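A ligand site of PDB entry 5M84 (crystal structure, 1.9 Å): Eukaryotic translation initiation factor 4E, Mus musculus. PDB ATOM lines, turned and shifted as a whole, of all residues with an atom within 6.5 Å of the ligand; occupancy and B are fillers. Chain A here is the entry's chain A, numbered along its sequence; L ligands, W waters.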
ATOM      1  N   PHE A  21       2.600  -8.698   3.175  1.00  0.00           N
ATOM      2  CA  PHE A  21       1.631  -7.708   3.613  1.00  0.00           C
ATOM      3  C   PHE A  21       0.332  -8.443   3.808  1.00  0.00           C
ATOM      4  O   PHE A  21      -0.071  -9.266   2.972  1.00  0.00           O
ATOM      5  CB  PHE A  21       1.449  -6.595   2.578  1.00  0.00           C
ATOM      6  CG  PHE A  21       0.338  -5.612   2.928  1.00  0.00           C
ATOM      7  CD1 PHE A  21      -0.978  -5.893   2.589  1.00  0.00           C
ATOM      8  CD2 PHE A  21       0.632  -4.427   3.579  1.00  0.00           C
ATOM      9  CE1 PHE A  21      -1.997  -5.014   2.919  1.00  0.00           C
ATOM     10  CE2 PHE A  21      -0.394  -3.519   3.914  1.00  0.00           C
ATOM     11  CZ  PHE A  21      -1.700  -3.823   3.577  1.00  0.00           C
ATOM     12  N   ASN A  23      -3.620  -7.422   4.844  1.00  0.00           N
ATOM     13  CA  ASN A  23      -4.516  -6.351   5.228  1.00  0.00           C
ATOM     14  C   ASN A  23      -5.115  -6.693   6.576  1.00  0.00           C
ATOM     15  O   ASN A  23      -5.664  -7.779   6.798  1.00  0.00           O
ATOM     16  CB  ASN A  23      -5.608  -6.094   4.177  1.00  0.00           C
ATOM     17  CG  ASN A  23      -6.157  -4.676   4.298  1.00  0.00           C
ATOM     18  OD1 ASN A  23      -5.534  -3.810   4.917  1.00  0.00           O
ATOM     19  ND2 ASN A  23      -7.344  -4.445   3.753  1.00  0.00           N
ATOM     20  N   TRP A  29      -1.315   0.975   7.170  1.00  0.00           N
ATOM     21  CA  TRP A  29      -0.776   0.232   6.035  1.00  0.00           C
ATOM     22  C   TRP A  29       0.666  -0.162   6.281  1.00  0.00           C
ATOM     23  O   TRP A  29       1.050  -1.317   6.104  1.00  0.00           O
ATOM     24  CB  TRP A  29      -0.871   1.081   4.744  1.00  0.00           C
ATOM     25  CG  TRP A  29      -0.363   0.348   3.509  1.00  0.00           C
ATOM     26  CD1 TRP A  29      -1.091  -0.446   2.681  1.00  0.00           C
ATOM     27  CD2 TRP A  29       0.977   0.360   2.983  1.00  0.00           C
ATOM     28  NE1 TRP A  29      -0.289  -0.952   1.672  1.00  0.00           N
ATOM     29  CE2 TRP A  29       0.990  -0.459   1.847  1.00  0.00           C
ATOM     30  CE3 TRP A  29       2.166   0.971   3.384  1.00  0.00           C
ATOM     31  CZ2 TRP A  29       2.146  -0.689   1.090  1.00  0.00           C
ATOM     32  CZ3 TRP A  29       3.322   0.763   2.623  1.00  0.00           C
ATOM     33  CH2 TRP A  29       3.298  -0.062   1.502  1.00  0.00           C
ATOM     34  N   GLN A  30       1.495   0.780   6.752  1.00  0.00           N
ATOM     35  CA  GLN A  30       2.902   0.479   6.961  1.00  0.00           C
ATOM     36  C   GLN A  30       3.102  -0.596   8.027  1.00  0.00           C
ATOM     37  O   GLN A  30       3.989  -1.450   7.890  1.00  0.00           O
ATOM     38  CB  GLN A  30       3.674   1.738   7.345  1.00  0.00           C
ATOM     39  CG  GLN A  30       3.777   2.771   6.223  1.00  0.00           C
ATOM     40  N   GLY A  61      -6.280  -9.606  -0.080  1.00  0.00           N
ATOM     41  CA  GLY A  61      -5.739  -8.555   0.739  1.00  0.00           C
ATOM     42  C   GLY A  61      -4.302  -8.750   1.155  1.00  0.00           C
ATOM     43  O   GLY A  61      -3.782  -7.949   1.926  1.00  0.00           O
ATOM     44  N   ASP A  63      -0.103  -9.240   0.074  1.00  0.00           N
ATOM     45  CA  ASP A  63       0.874  -9.008  -0.977  1.00  0.00           C
ATOM     46  C   ASP A  63       2.171  -9.751  -0.673  1.00  0.00           C
ATOM     47  O   ASP A  63       2.540  -9.957   0.482  1.00  0.00           O
ATOM     48  CB  ASP A  63       1.307  -7.536  -1.197  1.00  0.00           C
ATOM     49  CG  ASP A  63       0.200  -6.545  -1.109  1.00  0.00           C
ATOM     50  OD1 ASP A  63       0.523  -5.394  -0.697  1.00  0.00           O
ATOM     51  OD2 ASP A  63      -0.931  -6.843  -1.534  1.00  0.00           O
ATOM     52  N   PRO A  73       9.468  -1.705   0.189  1.00  0.00           N
ATOM     53  CA  PRO A  73       8.489  -1.707  -0.910  1.00  0.00           C
ATOM     54  C   PRO A  73       7.389  -0.676  -0.701  1.00  0.00           C
ATOM     55  O   PRO A  73       6.203  -0.996  -0.672  1.00  0.00           O
ATOM     56  CB  PRO A  73       7.974  -3.155  -0.881  1.00  0.00           C
ATOM     57  CG  PRO A  73       8.303  -3.687   0.481  1.00  0.00           C
ATOM     58  CD  PRO A  73       9.178  -2.739   1.206  1.00  0.00           C
ATOM     59  N   MET A  74       7.785   0.595  -0.629  1.00  0.00           N
ATOM     60  CA  MET A  74       6.809   1.666  -0.470  1.00  0.00           C
ATOM     61  C   MET A  74       7.271   2.878  -1.254  1.00  0.00           C
ATOM     62  O   MET A  74       8.474   3.092  -1.464  1.00  0.00           O
ATOM     63  CB  MET A  74       6.587   2.030   1.014  1.00  0.00           C
ATOM     64  CG  MET A  74       7.841   2.419   1.749  1.00  0.00           C
ATOM     65  SD  MET A  74       7.554   2.619   3.529  1.00  0.00           S
ATOM     66  CE  MET A  74       7.213   0.953   4.014  1.00  0.00           C
ATOM     67  N   TRP A  75       6.286   3.643  -1.732  1.00  0.00           N
ATOM     68  CA  TRP A  75       6.547   4.859  -2.495  1.00  0.00           C
ATOM     69  C   TRP A  75       7.599   5.739  -1.840  1.00  0.00           C
ATOM     70  O   TRP A  75       8.406   6.354  -2.526  1.00  0.00           O
ATOM     71  CB  TRP A  75       5.262   5.662  -2.668  1.00  0.00           C
ATOM     72  CG  TRP A  75       4.146   4.915  -3.267  1.00  0.00           C
ATOM     73  CD1 TRP A  75       4.222   3.924  -4.223  1.00  0.00           C
ATOM     74  CD2 TRP A  75       2.769   5.054  -2.937  1.00  0.00           C
ATOM     75  NE1 TRP A  75       2.951   3.460  -4.512  1.00  0.00           N
ATOM     76  CE2 TRP A  75       2.043   4.142  -3.739  1.00  0.00           C
ATOM     77  CE3 TRP A  75       2.066   5.870  -2.049  1.00  0.00           C
ATOM     78  CZ2 TRP A  75       0.658   4.025  -3.673  1.00  0.00           C
ATOM     79  CZ3 TRP A  75       0.694   5.758  -1.977  1.00  0.00           C
ATOM     80  CH2 TRP A  75      -0.004   4.845  -2.786  1.00  0.00           C
ATOM     81  N   GLU A  76       7.556   5.855  -0.520  1.00  0.00           N
ATOM     82  CA  GLU A  76       8.325   6.878   0.174  1.00  0.00           C
ATOM     83  C   GLU A  76       9.821   6.585   0.226  1.00  0.00           C
ATOM     84  O   GLU A  76      10.612   7.475   0.580  1.00  0.00           O
ATOM     85  CB  GLU A  76       7.761   7.092   1.576  1.00  0.00           C
ATOM     86  CG  GLU A  76       6.301   7.572   1.603  1.00  0.00           C
ATOM     87  CD  GLU A  76       5.265   6.458   1.714  1.00  0.00           C
ATOM     88  OE1 GLU A  76       4.246   6.688   2.398  1.00  0.00           O
ATOM     89  OE2 GLU A  76       5.450   5.357   1.134  1.00  0.00           O
ATOM     90  N   ARG A  85       5.886   2.036 -11.861  1.00  0.00           N
ATOM     91  CA  ARG A  85       5.731   0.595 -12.018  1.00  0.00           C
ATOM     92  C   ARG A  85       5.150   0.236 -13.381  1.00  0.00           C
ATOM     93  O   ARG A  85       4.237   0.907 -13.881  1.00  0.00           O
ATOM     94  CB  ARG A  85       4.839   0.002 -10.931  1.00  0.00           C
ATOM     95  CG  ARG A  85       3.407   0.525 -10.969  1.00  0.00           C
ATOM     96  CD  ARG A  85       2.549  -0.087  -9.863  1.00  0.00           C
ATOM     97  NE  ARG A  85       1.168   0.418  -9.900  1.00  0.00           N
ATOM     98  CZ  ARG A  85       0.184  -0.034  -9.116  1.00  0.00           C
ATOM     99  NH1 ARG A  85      -1.029   0.483  -9.231  1.00  0.00           N
ATOM    100  NH2 ARG A  85       0.411  -1.001  -8.229  1.00  0.00           N
ATOM    101  N   ASN A 128      -0.159  -8.185  -5.785  1.00  0.00           N
ATOM    102  CA  ASN A 128      -1.303  -7.919  -4.930  1.00  0.00           C
ATOM    103  C   ASN A 128      -2.389  -8.943  -5.248  1.00  0.00           C
ATOM    104  O   ASN A 128      -2.848  -9.025  -6.391  1.00  0.00           O
ATOM    105  CB  ASN A 128      -1.868  -6.501  -5.113  1.00  0.00           C
ATOM    106  CG  ASN A 128      -0.793  -5.422  -5.040  1.00  0.00           C
ATOM    107  OD1 ASN A 128      -0.296  -5.119  -3.959  1.00  0.00           O
ATOM    108  ND2 ASN A 128      -0.503  -4.787  -6.175  1.00  0.00           N
ATOM    109  N   VAL A 129      -2.794  -9.702  -4.246  1.00  0.00           N
ATOM    110  CA  VAL A 129      -3.910 -10.631  -4.346  1.00  0.00           C
ATOM    111  C   VAL A 129      -5.139  -9.927  -3.779  1.00  0.00           C
ATOM    112  O   VAL A 129      -5.150  -9.522  -2.597  1.00  0.00           O
ATOM    113  CB  VAL A 129      -3.625 -11.950  -3.592  1.00  0.00           C
ATOM    114  CG1 VAL A 129      -4.800 -12.921  -3.722  1.00  0.00           C
ATOM    115  CG2 VAL A 129      -2.336 -12.552  -4.097  1.00  0.00           C
ATOM    116  N   ARG A 130      -6.180  -9.787  -4.625  1.00  0.00           N
ATOM    117  CA  ARG A 130      -7.384  -9.040  -4.276  1.00  0.00           C
ATOM    118  C   ARG A 130      -8.615  -9.732  -4.849  1.00  0.00           C
ATOM    119  O   ARG A 130      -8.565 -10.380  -5.894  1.00  0.00           O
ATOM    120  CB  ARG A 130      -7.369  -7.603  -4.850  1.00  0.00           C
ATOM    121  CG  ARG A 130      -6.242  -6.705  -4.370  1.00  0.00           C
ATOM    122  CD  ARG A 130      -6.316  -6.473  -2.886  1.00  0.00           C
ATOM    123  NE  ARG A 130      -5.257  -5.530  -2.487  1.00  0.00           N
ATOM    124  CZ  ARG A 130      -4.063  -5.894  -2.022  1.00  0.00           C
ATOM    125  NH1 ARG A 130      -3.780  -7.184  -1.891  1.00  0.00           N
ATOM    126  NH2 ARG A 130      -3.177  -4.962  -1.712  1.00  0.00           N
ATOM    127  N   LYS A 132     -11.076  -8.180  -6.171  1.00  0.00           N
ATOM    128  CA  LYS A 132     -11.470  -7.431  -7.362  1.00  0.00           C
ATOM    129  C   LYS A 132     -10.590  -7.693  -8.576  1.00  0.00           C
ATOM    130  O   LYS A 132     -10.936  -7.232  -9.675  1.00  0.00           O
ATOM    131  CB  LYS A 132     -11.477  -5.925  -7.073  1.00  0.00           C
ATOM    132  N   GLY A 133      -9.489  -8.416  -8.417  1.00  0.00           N
ATOM    133  CA  GLY A 133      -8.547  -8.666  -9.490  1.00  0.00           C
ATOM    134  C   GLY A 133      -7.099  -8.480  -9.047  1.00  0.00           C
ATOM    135  O   GLY A 133      -6.769  -7.449  -8.442  1.00  0.00           O
ATOM    136  N   LYS A 135      -2.823  -8.092  -9.200  1.00  0.00           N
ATOM    137  CA  LYS A 135      -1.902  -7.191  -9.889  1.00  0.00           C
ATOM    138  C   LYS A 135      -0.492  -7.687  -9.673  1.00  0.00           C
ATOM    139  O   LYS A 135      -0.136  -8.148  -8.577  1.00  0.00           O
ATOM    140  CB  LYS A 135      -2.030  -5.747  -9.393  1.00  0.00           C
ATOM    141  CG  LYS A 135      -3.417  -5.175  -9.610  1.00  0.00           C
ATOM    142  CD  LYS A 135      -3.331  -3.692  -9.827  1.00  0.00           C
ATOM    143  CE  LYS A 135      -3.648  -2.932  -8.569  1.00  0.00           C
ATOM    144  NZ  LYS A 135      -5.110  -2.882  -8.329  1.00  0.00           N
ATOM    145  N   TRP A 139       8.713  -2.391 -10.104  1.00  0.00           N
ATOM    146  CA  TRP A 139       9.014  -1.031  -9.692  1.00  0.00           C
ATOM    147  C   TRP A 139      10.412  -0.637 -10.164  1.00  0.00           C
ATOM    148  O   TRP A 139      11.379  -1.393  -9.959  1.00  0.00           O
ATOM    149  CB  TRP A 139       8.935  -0.883  -8.168  1.00  0.00           C
ATOM    150  CG  TRP A 139       7.552  -1.007  -7.585  1.00  0.00           C
ATOM    151  CD1 TRP A 139       6.483  -1.701  -8.120  1.00  0.00           C
ATOM    152  CD2 TRP A 139       7.072  -0.385  -6.386  1.00  0.00           C
ATOM    153  NE1 TRP A 139       5.385  -1.576  -7.310  1.00  0.00           N
ATOM    154  CE2 TRP A 139       5.715  -0.765  -6.242  1.00  0.00           C
ATOM    155  CE3 TRP A 139       7.669   0.426  -5.411  1.00  0.00           C
ATOM    156  CZ2 TRP A 139       4.954  -0.335  -5.173  1.00  0.00           C
ATOM    157  CZ3 TRP A 139       6.904   0.845  -4.358  1.00  0.00           C
ATOM    158  CH2 TRP A 139       5.560   0.468  -4.245  1.00  0.00           C
ATOM    159  N   THR A 176       0.002   7.539  -8.577  1.00  0.00           N
ATOM    160  CA  THR A 176      -0.724   6.553  -7.782  1.00  0.00           C
ATOM    161  C   THR A 176      -1.064   7.089  -6.399  1.00  0.00           C
ATOM    162  O   THR A 176      -2.183   6.916  -5.909  1.00  0.00           O
ATOM    163  CB  THR A 176       0.112   5.288  -7.655  1.00  0.00           C
ATOM    164  OG1 THR A 176       0.569   4.881  -8.948  1.00  0.00           O
ATOM    165  CG2 THR A 176      -0.698   4.150  -7.019  1.00  0.00           C
HETATM  166  C1  LIG L   1       1.915   4.306   1.518  1.00  0.00           C
HETATM  167  C2  LIG L   1      -0.219   1.283  -0.949  1.00  0.00           C
HETATM  168  C3  LIG L   1       0.494   2.819   0.419  1.00  0.00           C
HETATM  169  C4  LIG L   1       1.544   2.386  -0.361  1.00  0.00           C
HETATM  170  C5  LIG L   1       2.814   2.937  -0.191  1.00  0.00           C
HETATM  171  O1  LIG L   1      -7.956  -3.254  -1.864  1.00  0.00           O
HETATM  172  P1  LIG L   1      -7.589  -2.419  -3.197  1.00  0.00           P
HETATM  173  O2  LIG L   1      -8.280  -1.075  -3.189  1.00  0.00           O
HETATM  174  O3  LIG L   1      -8.003  -3.210  -4.413  1.00  0.00           O
HETATM  175  O4  LIG L   1      -6.001  -2.167  -3.198  1.00  0.00           O
HETATM  176  P2  LIG L   1      -5.219  -1.927  -4.579  1.00  0.00           P
HETATM  177  O5  LIG L   1      -6.101  -1.364  -5.621  1.00  0.00           O
HETATM  178  S1  LIG L   1      -4.398  -3.724  -5.210  1.00  0.00           S
HETATM  179  O6  LIG L   1      -4.077  -0.838  -4.299  1.00  0.00           O
HETATM  180  P3  LIG L   1      -3.002  -0.984  -3.111  1.00  0.00           P
HETATM  181  O7  LIG L   1      -3.343  -2.060  -2.127  1.00  0.00           O
HETATM  182  O8  LIG L   1      -1.632  -1.130  -3.704  1.00  0.00           O
HETATM  183  O9  LIG L   1      -3.073   0.412  -2.299  1.00  0.00           O
HETATM  184  C6  LIG L   1      -4.210   0.671  -1.505  1.00  0.00           C
HETATM  185  C7  LIG L   1      -3.823   1.746  -0.511  1.00  0.00           C
HETATM  186  O10 LIG L   1      -2.777   1.255   0.332  1.00  0.00           O
HETATM  187  C8  LIG L   1      -3.245   2.963  -1.188  1.00  0.00           C
HETATM  188  O11 LIG L   1      -4.285   3.831  -1.652  1.00  0.00           O
HETATM  189  C9  LIG L   1      -2.438   3.566  -0.055  1.00  0.00           C
HETATM  190  O12 LIG L   1      -3.257   4.319   0.834  1.00  0.00           O
HETATM  191  C10 LIG L   1      -2.526   5.350   1.492  1.00  0.00           C
HETATM  192  C11 LIG L   1      -1.904   2.329   0.652  1.00  0.00           C
HETATM  193  N1  LIG L   1      -0.569   2.123   0.050  1.00  0.00           N
HETATM  194  N2  LIG L   1       1.093   1.447  -1.212  1.00  0.00           N
HETATM  195  C12 LIG L   1       1.846   0.684  -2.256  1.00  0.00           C
HETATM  196  N3  LIG L   1       0.690   3.771   1.362  1.00  0.00           N
HETATM  197  N4  LIG L   1       2.090   5.267   2.460  1.00  0.00           N
HETATM  198  N5  LIG L   1       2.959   3.907   0.752  1.00  0.00           N
HETATM  199  O13 LIG L   1       3.900   2.572  -0.917  1.00  0.00           O
HETATM  200  O   HOH W   1      -8.415   0.149  -5.898  1.00  0.00           O
HETATM  201  O   HOH W   2      -1.456   1.136  -5.195  1.00  0.00           O
HETATM  202  O   HOH W   3      -3.151   0.567  -7.157  1.00  0.00           O
HETATM  203  O   HOH W   4      -0.686  -3.068  -0.436  1.00  0.00           O
HETATM  204  O   HOH W   5      -1.247  -2.140  -6.096  1.00  0.00           O
HETATM  205  O   HOH W   6      -3.470   3.274  -4.550  1.00  0.00           O
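The side-chain carboxylate of Glu 76 is in hydrogen-bond range of a nitrogen (N4) of the ligand. N of Trp 75 lies within hydrogen-bond range of O13 of the ligand, 2.7 Å away. The side-chain amino group of Lys 135 is in hydrogen-bond range of an oxygen (O5) of the ligand (3.3 Å). The guanidinium group (NH2) of Arg 130 lies within salt-bridge range of an oxygen (O7) of the ligand, 2.9 Å away.
Water W5 lies within hydrogen-bond range of O8 of the ligand, ND2 of Asn 128 and NH2 of Arg 85. Water W4 lies within hydrogen-bond range of OD1 of Asp 63 (2.6 Å), NE1 of Trp 29 (3.0 Å), O7 of the ligand (3.3 Å) and NH2 of Arg 130 (3.4 Å). Water W3 bridges the guanidinium group (NH1) of Arg 85 and an oxygen (O6) of the ligand.
N1 of the ligand lies close to NE1 of Trp 29, 3.5 Å away. Met 74 touches the ligand (CA to O13, 3.1 Å). Asn 128 touches the ligand (CB to S1, 3.8 Å). Hydrophobic or aromatic side chains within 4 Å of the ligand: Trp 29, Met 74 and Trp 75. Of the 19 residues printed, 7 come within 4 Å of the ligand. Along chain A the residues within 4 Å of the ligand span positions 29 to 135.
NH1 of Arg 130 is in salt-bridge range of OD2 of Asp 63. The side-chain amide oxygen (OD1) of Asn 128 lies close to the side-chain carboxylate (OD2) of Asp 63 (3.0 Å). O of Lys 135 lies within hydrogen-bond range of N of Asn 128 (2.8 Å).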
